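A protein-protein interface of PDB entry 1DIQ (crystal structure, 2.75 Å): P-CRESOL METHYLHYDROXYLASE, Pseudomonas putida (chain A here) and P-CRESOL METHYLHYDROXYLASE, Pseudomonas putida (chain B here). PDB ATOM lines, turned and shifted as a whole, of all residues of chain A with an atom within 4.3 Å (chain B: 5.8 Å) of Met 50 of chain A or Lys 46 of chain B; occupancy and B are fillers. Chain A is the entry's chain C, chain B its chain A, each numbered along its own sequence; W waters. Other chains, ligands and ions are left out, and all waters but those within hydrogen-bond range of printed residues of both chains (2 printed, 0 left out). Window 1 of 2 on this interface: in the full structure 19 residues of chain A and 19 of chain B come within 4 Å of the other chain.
Among the printed residues, pairs that only touch across the chains: Asn 45 of chain A with Val 42 of chain B, Met 50 of chain A with Lys 46 of chain B, Arg 48 of chain A with Gly 390 of chain B, Ala 52 of chain A with Pro 43 of chain B, Asn 45 of chain A with Lys 46 of chain B, Ala 49 of chain A with Gly 390 of chain B and Gly 46 of chain A with Lys 46 of chain B.
Met 50 of chain A touches just one residue of chain B: Lys 46. Printed residues of chain A within 4 Å of Lys 46 of chain B: Asn 45, Gly 46, Arg 48 and Met 50. Printed residues of chain A within 4 Å of Val 42 of chain B: Asn 45. Of the printed residues of chain A, Gly 390 of chain B touches Arg 48 and Ala 49. Of the printed residues of chain B, Ala 52 of chain A touches Pro 43 (3.5 Å). Printed residues of chain B within 4 Å of Arg 48 of chain A: Lys 46 (2.5 Å) and Gly 390 (3.4 Å). Of the printed residues of chain A, Pro 43 of chain B touches Ala 52 (3.5 Å). Ile 47 of chain B touches none of the printed residues of chain A.
Hydrophobic or aromatic side chains of chain B that line the printed part of chain A: Val 42 and Pro 43. Printed residues of chain A that touch a printed residue of chain B: Asn 45, Gly 46, Arg 48, Ala 49, Met 50 and Ala 52. Hydrophobic or aromatic side chains of chain A that line the printed part of chain B: Ala 52. Among the printed residues, 8 pairs touch across the chains. Among the printed residues, no Asp or Glu carboxylate lies within 4 Å of a Lys or Arg side-chain nitrogen of the other chain.
The side-chain amino group (NZ) of Lys 46 of chain B lies within hydrogen-bond range of the backbone carbonyl oxygen (O) of Arg 48 of chain A (2.5 Å).
Water W1 lies within hydrogen-bond range of the backbone carbonyl oxygen of Pro 43 of chain B (2.5 Å) and the backbone carbonyl oxygen of Ala 52 of chain A (3.0 Å). Water W2 bridges the backbone carbonyl oxygen of Ala 49 of chain A (2.6 Å) and the side-chain sulfur of Met 48 of chain B (3.6 Å).
The side-chain hydroxyl (OG) of Ser 97 of chain B sits close to the backbone carbonyl oxygen (O) of Lys 46 of chain B (3.5 Å).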
ATOM      1  N   ILE A  42       4.602 -32.746 -19.687  1.00  0.00           N
ATOM      2  CA  ILE A  42       5.146 -31.402 -19.776  1.00  0.00           C
ATOM      3  C   ILE A  42       6.004 -31.071 -18.561  1.00  0.00           C
ATOM      4  O   ILE A  42       7.067 -30.487 -18.715  1.00  0.00           O
ATOM      5  CB  ILE A  42       4.017 -30.339 -19.982  1.00  0.00           C
ATOM      6  CG1 ILE A  42       3.342 -30.544 -21.334  1.00  0.00           C
ATOM      7  CG2 ILE A  42       4.549 -28.921 -19.938  1.00  0.00           C
ATOM      8  CD1 ILE A  42       4.294 -30.656 -22.565  1.00  0.00           C
ATOM      9  N   VAL A  43       5.580 -31.492 -17.367  1.00  0.00           N
ATOM     10  CA  VAL A  43       6.341 -31.205 -16.152  1.00  0.00           C
ATOM     11  C   VAL A  43       7.605 -32.046 -16.066  1.00  0.00           C
ATOM     12  O   VAL A  43       8.651 -31.546 -15.671  1.00  0.00           O
ATOM     13  CB  VAL A  43       5.463 -31.307 -14.895  1.00  0.00           C
ATOM     14  CG1 VAL A  43       6.246 -31.062 -13.616  1.00  0.00           C
ATOM     15  CG2 VAL A  43       4.424 -30.268 -14.971  1.00  0.00           C
ATOM     16  N   ASN A  45       9.212 -33.480 -18.809  1.00  0.00           N
ATOM     17  CA  ASN A  45      10.114 -33.204 -19.934  1.00  0.00           C
ATOM     18  C   ASN A  45      10.449 -31.742 -20.070  1.00  0.00           C
ATOM     19  O   ASN A  45      11.544 -31.388 -20.496  1.00  0.00           O
ATOM     20  CB  ASN A  45       9.534 -33.704 -21.268  1.00  0.00           C
ATOM     21  CG  ASN A  45       9.587 -35.216 -21.407  1.00  0.00           C
ATOM     22  OD1 ASN A  45      10.549 -35.764 -21.929  1.00  0.00           O
ATOM     23  ND2 ASN A  45       8.546 -35.893 -20.950  1.00  0.00           N
ATOM     24  N   GLY A  46       9.499 -30.893 -19.695  1.00  0.00           N
ATOM     25  CA  GLY A  46       9.663 -29.459 -19.827  1.00  0.00           C
ATOM     26  C   GLY A  46       9.248 -29.136 -21.253  1.00  0.00           C
ATOM     27  O   GLY A  46       9.382 -29.983 -22.147  1.00  0.00           O
ATOM     28  N   PHE A  47       8.715 -27.942 -21.485  1.00  0.00           N
ATOM     29  CA  PHE A  47       8.320 -27.601 -22.838  1.00  0.00           C
ATOM     30  C   PHE A  47       8.824 -26.234 -23.263  1.00  0.00           C
ATOM     31  O   PHE A  47       8.239 -25.207 -22.897  1.00  0.00           O
ATOM     32  CB  PHE A  47       6.801 -27.726 -23.013  1.00  0.00           C
ATOM     33  CG  PHE A  47       6.339 -27.533 -24.425  1.00  0.00           C
ATOM     34  CD1 PHE A  47       6.899 -28.300 -25.475  1.00  0.00           C
ATOM     35  CD2 PHE A  47       5.407 -26.524 -24.728  1.00  0.00           C
ATOM     36  CE1 PHE A  47       6.547 -28.057 -26.815  1.00  0.00           C
ATOM     37  CE2 PHE A  47       5.034 -26.262 -26.069  1.00  0.00           C
ATOM     38  CZ  PHE A  47       5.613 -27.034 -27.117  1.00  0.00           C
ATOM     39  N   ARG A  48       9.860 -26.254 -24.108  1.00  0.00           N
ATOM     40  CA  ARG A  48      10.515 -25.063 -24.653  1.00  0.00           C
ATOM     41  C   ARG A  48      10.928 -24.086 -23.544  1.00  0.00           C
ATOM     42  O   ARG A  48      11.909 -24.324 -22.840  1.00  0.00           O
ATOM     43  CB  ARG A  48       9.621 -24.337 -25.673  1.00  0.00           C
ATOM     44  CG  ARG A  48       9.229 -25.058 -26.945  1.00  0.00           C
ATOM     45  CD  ARG A  48       8.502 -24.032 -27.782  1.00  0.00           C
ATOM     46  NE  ARG A  48       7.704 -24.555 -28.887  1.00  0.00           N
ATOM     47  CZ  ARG A  48       6.435 -24.220 -29.110  1.00  0.00           C
ATOM     48  NH1 ARG A  48       5.799 -23.374 -28.291  1.00  0.00           N
ATOM     49  NH2 ARG A  48       5.810 -24.700 -30.183  1.00  0.00           N
ATOM     50  N   ALA A  49      10.145 -23.013 -23.378  1.00  0.00           N
ATOM     51  CA  ALA A  49      10.378 -21.963 -22.374  1.00  0.00           C
ATOM     52  C   ALA A  49      10.130 -22.448 -20.945  1.00  0.00           C
ATOM     53  O   ALA A  49      10.696 -21.904 -19.989  1.00  0.00           O
ATOM     54  CB  ALA A  49       9.514 -20.744 -22.688  1.00  0.00           C
ATOM     55  N   MET A  50       9.290 -23.479 -20.819  1.00  0.00           N
ATOM     56  CA  MET A  50       8.972 -24.081 -19.531  1.00  0.00           C
ATOM     57  C   MET A  50      10.052 -25.027 -18.989  1.00  0.00           C
ATOM     58  O   MET A  50      10.541 -25.913 -19.700  1.00  0.00           O
ATOM     59  CB  MET A  50       7.651 -24.882 -19.571  1.00  0.00           C
ATOM     60  CG  MET A  50       7.250 -25.339 -18.149  1.00  0.00           C
ATOM     61  SD  MET A  50       5.685 -25.972 -17.751  1.00  0.00           S
ATOM     62  CE  MET A  50       6.177 -27.251 -16.690  1.00  0.00           C
ATOM     63  N   PRO A  51      10.430 -24.850 -17.709  1.00  0.00           N
ATOM     64  CA  PRO A  51      11.435 -25.746 -17.132  1.00  0.00           C
ATOM     65  C   PRO A  51      10.821 -27.113 -16.769  1.00  0.00           C
ATOM     66  O   PRO A  51       9.606 -27.285 -16.774  1.00  0.00           O
ATOM     67  CB  PRO A  51      11.850 -25.003 -15.866  1.00  0.00           C
ATOM     68  CG  PRO A  51      10.653 -24.183 -15.501  1.00  0.00           C
ATOM     69  CD  PRO A  51      10.234 -23.665 -16.844  1.00  0.00           C
ATOM     70  N   ALA A  52      11.676 -28.093 -16.508  1.00  0.00           N
ATOM     71  CA  ALA A  52      11.235 -29.421 -16.092  1.00  0.00           C
ATOM     72  C   ALA A  52      11.484 -29.524 -14.604  1.00  0.00           C
ATOM     73  O   ALA A  52      12.425 -28.914 -14.091  1.00  0.00           O
ATOM     74  CB  ALA A  52      12.008 -30.467 -16.806  1.00  0.00           C
ATOM     75  N   VAL B  42      15.028 -37.836 -17.384  1.00  0.00           N
ATOM     76  CA  VAL B  42      14.642 -36.806 -18.346  1.00  0.00           C
ATOM     77  C   VAL B  42      14.454 -35.363 -17.798  1.00  0.00           C
ATOM     78  O   VAL B  42      14.867 -34.411 -18.470  1.00  0.00           O
ATOM     79  CB  VAL B  42      13.480 -37.345 -19.281  1.00  0.00           C
ATOM     80  CG1 VAL B  42      12.436 -36.313 -19.587  1.00  0.00           C
ATOM     81  CG2 VAL B  42      14.075 -37.842 -20.566  1.00  0.00           C
ATOM     82  N   PRO B  43      13.849 -35.177 -16.590  1.00  0.00           N
ATOM     83  CA  PRO B  43      13.713 -33.793 -16.113  1.00  0.00           C
ATOM     84  C   PRO B  43      15.002 -33.071 -15.687  1.00  0.00           C
ATOM     85  O   PRO B  43      15.026 -31.847 -15.566  1.00  0.00           O
ATOM     86  CB  PRO B  43      12.700 -33.919 -14.960  1.00  0.00           C
ATOM     87  CG  PRO B  43      12.836 -35.288 -14.516  1.00  0.00           C
ATOM     88  CD  PRO B  43      12.987 -36.060 -15.777  1.00  0.00           C
ATOM     89  N   TYR B  44      16.065 -33.836 -15.477  1.00  0.00           N
ATOM     90  CA  TYR B  44      17.364 -33.295 -15.095  1.00  0.00           C
ATOM     91  C   TYR B  44      18.159 -32.842 -16.329  1.00  0.00           C
ATOM     92  O   TYR B  44      19.076 -32.023 -16.227  1.00  0.00           O
ATOM     93  CB  TYR B  44      18.178 -34.362 -14.378  1.00  0.00           C
ATOM     94  CG  TYR B  44      17.657 -34.789 -13.031  1.00  0.00           C
ATOM     95  CD1 TYR B  44      17.861 -33.997 -11.884  1.00  0.00           C
ATOM     96  CD2 TYR B  44      17.013 -36.026 -12.877  1.00  0.00           C
ATOM     97  CE1 TYR B  44      17.438 -34.441 -10.603  1.00  0.00           C
ATOM     98  CE2 TYR B  44      16.578 -36.481 -11.610  1.00  0.00           C
ATOM     99  CZ  TYR B  44      16.793 -35.687 -10.482  1.00  0.00           C
ATOM    100  OH  TYR B  44      16.336 -36.128  -9.265  1.00  0.00           O
ATOM    101  N   ASN B  45      17.782 -33.380 -17.487  1.00  0.00           N
ATOM    102  CA  ASN B  45      18.442 -33.103 -18.752  1.00  0.00           C
ATOM    103  C   ASN B  45      18.047 -31.807 -19.445  1.00  0.00           C
ATOM    104  O   ASN B  45      18.787 -31.352 -20.313  1.00  0.00           O
ATOM    105  CB  ASN B  45      18.209 -34.269 -19.718  1.00  0.00           C
ATOM    106  CG  ASN B  45      19.470 -34.691 -20.472  1.00  0.00           C
ATOM    107  OD1 ASN B  45      19.625 -35.872 -20.790  1.00  0.00           O
ATOM    108  ND2 ASN B  45      20.357 -33.739 -20.784  1.00  0.00           N
ATOM    109  N   LYS B  46      16.916 -31.197 -19.087  1.00  0.00           N
ATOM    110  CA  LYS B  46      16.521 -29.955 -19.766  1.00  0.00           C
ATOM    111  C   LYS B  46      17.474 -28.753 -19.625  1.00  0.00           C
ATOM    112  O   LYS B  46      17.736 -28.247 -18.531  1.00  0.00           O
ATOM    113  CB  LYS B  46      15.095 -29.530 -19.456  1.00  0.00           C
ATOM    114  CG  LYS B  46      14.535 -28.719 -20.617  1.00  0.00           C
ATOM    115  CD  LYS B  46      13.219 -28.073 -20.313  1.00  0.00           C
ATOM    116  CE  LYS B  46      12.684 -27.415 -21.557  1.00  0.00           C
ATOM    117  NZ  LYS B  46      13.354 -26.136 -21.809  1.00  0.00           N
ATOM    118  N   ILE B  47      18.053 -28.387 -20.771  1.00  0.00           N
ATOM    119  CA  ILE B  47      18.999 -27.288 -20.883  1.00  0.00           C
ATOM    120  C   ILE B  47      18.544 -26.257 -21.898  1.00  0.00           C
ATOM    121  O   ILE B  47      17.764 -26.564 -22.790  1.00  0.00           O
ATOM    122  CB  ILE B  47      20.414 -27.797 -21.248  1.00  0.00           C
ATOM    123  CG1 ILE B  47      20.370 -28.673 -22.510  1.00  0.00           C
ATOM    124  CG2 ILE B  47      21.021 -28.544 -20.045  1.00  0.00           C
ATOM    125  CD1 ILE B  47      21.713 -29.149 -22.990  1.00  0.00           C
ATOM    126  N   MET B  48      18.989 -25.017 -21.705  1.00  0.00           N
ATOM    127  CA  MET B  48      18.669 -23.895 -22.587  1.00  0.00           C
ATOM    128  C   MET B  48      19.937 -23.472 -23.343  1.00  0.00           C
ATOM    129  O   MET B  48      19.980 -22.402 -23.945  1.00  0.00           O
ATOM    130  CB  MET B  48      18.091 -22.717 -21.784  1.00  0.00           C
ATOM    131  CG  MET B  48      16.950 -23.078 -20.853  1.00  0.00           C
ATOM    132  SD  MET B  48      16.284 -21.650 -20.005  1.00  0.00           S
ATOM    133  CE  MET B  48      15.028 -21.150 -21.179  1.00  0.00           C
ATOM    134  N   ASN B  53      20.989 -32.432 -25.747  1.00  0.00           N
ATOM    135  CA  ASN B  53      20.856 -32.988 -24.409  1.00  0.00           C
ATOM    136  C   ASN B  53      21.873 -34.065 -24.049  1.00  0.00           C
ATOM    137  O   ASN B  53      22.340 -34.112 -22.911  1.00  0.00           O
ATOM    138  CB  ASN B  53      19.446 -33.533 -24.221  1.00  0.00           C
ATOM    139  CG  ASN B  53      18.391 -32.455 -24.289  1.00  0.00           C
ATOM    140  OD1 ASN B  53      18.635 -31.347 -24.784  1.00  0.00           O
ATOM    141  ND2 ASN B  53      17.200 -32.774 -23.795  1.00  0.00           N
ATOM    142  N   GLY B  96      23.294 -23.874 -17.044  1.00  0.00           N
ATOM    143  CA  GLY B  96      23.481 -25.323 -17.073  1.00  0.00           C
ATOM    144  C   GLY B  96      22.303 -26.119 -16.495  1.00  0.00           C
ATOM    145  O   GLY B  96      22.212 -27.345 -16.683  1.00  0.00           O
ATOM    146  N   SER B  97      21.360 -25.403 -15.868  1.00  0.00           N
ATOM    147  CA  SER B  97      20.180 -25.967 -15.201  1.00  0.00           C
ATOM    148  C   SER B  97      20.510 -27.012 -14.133  1.00  0.00           C
ATOM    149  O   SER B  97      21.259 -26.716 -13.200  1.00  0.00           O
ATOM    150  CB  SER B  97      19.124 -26.437 -16.196  1.00  0.00           C
ATOM    151  OG  SER B  97      18.476 -25.321 -16.776  1.00  0.00           O
ATOM    152  N   ALA B  98      19.984 -28.224 -14.274  1.00  0.00           N
ATOM    153  CA  ALA B  98      20.233 -29.279 -13.309  1.00  0.00           C
ATOM    154  C   ALA B  98      21.163 -30.325 -13.889  1.00  0.00           C
ATOM    155  O   ALA B  98      21.551 -31.256 -13.186  1.00  0.00           O
ATOM    156  CB  ALA B  98      18.943 -29.906 -12.901  1.00  0.00           C
ATOM    157  N   ALA B  99      21.547 -30.146 -15.155  1.00  0.00           N
ATOM    158  CA  ALA B  99      22.419 -31.085 -15.869  1.00  0.00           C
ATOM    159  C   ALA B  99      23.920 -30.926 -15.578  1.00  0.00           C
ATOM    160  O   ALA B  99      24.403 -29.804 -15.362  1.00  0.00           O
ATOM    161  CB  ALA B  99      22.168 -30.985 -17.355  1.00  0.00           C
ATOM    162  N   GLY B 390      12.910 -21.610 -25.995  1.00  0.00           N
ATOM    163  CA  GLY B 390      13.576 -22.135 -24.818  1.00  0.00           C
ATOM    164  C   GLY B 390      15.080 -22.085 -24.832  1.00  0.00           C
ATOM    165  O   GLY B 390      15.731 -22.910 -24.194  1.00  0.00           O
HETATM  166  O   HOH W   1      15.332 -29.671 -14.477  1.00  0.00           O
HETATM  167  O   HOH W   2      12.983 -22.529 -18.860  1.00  0.00           O
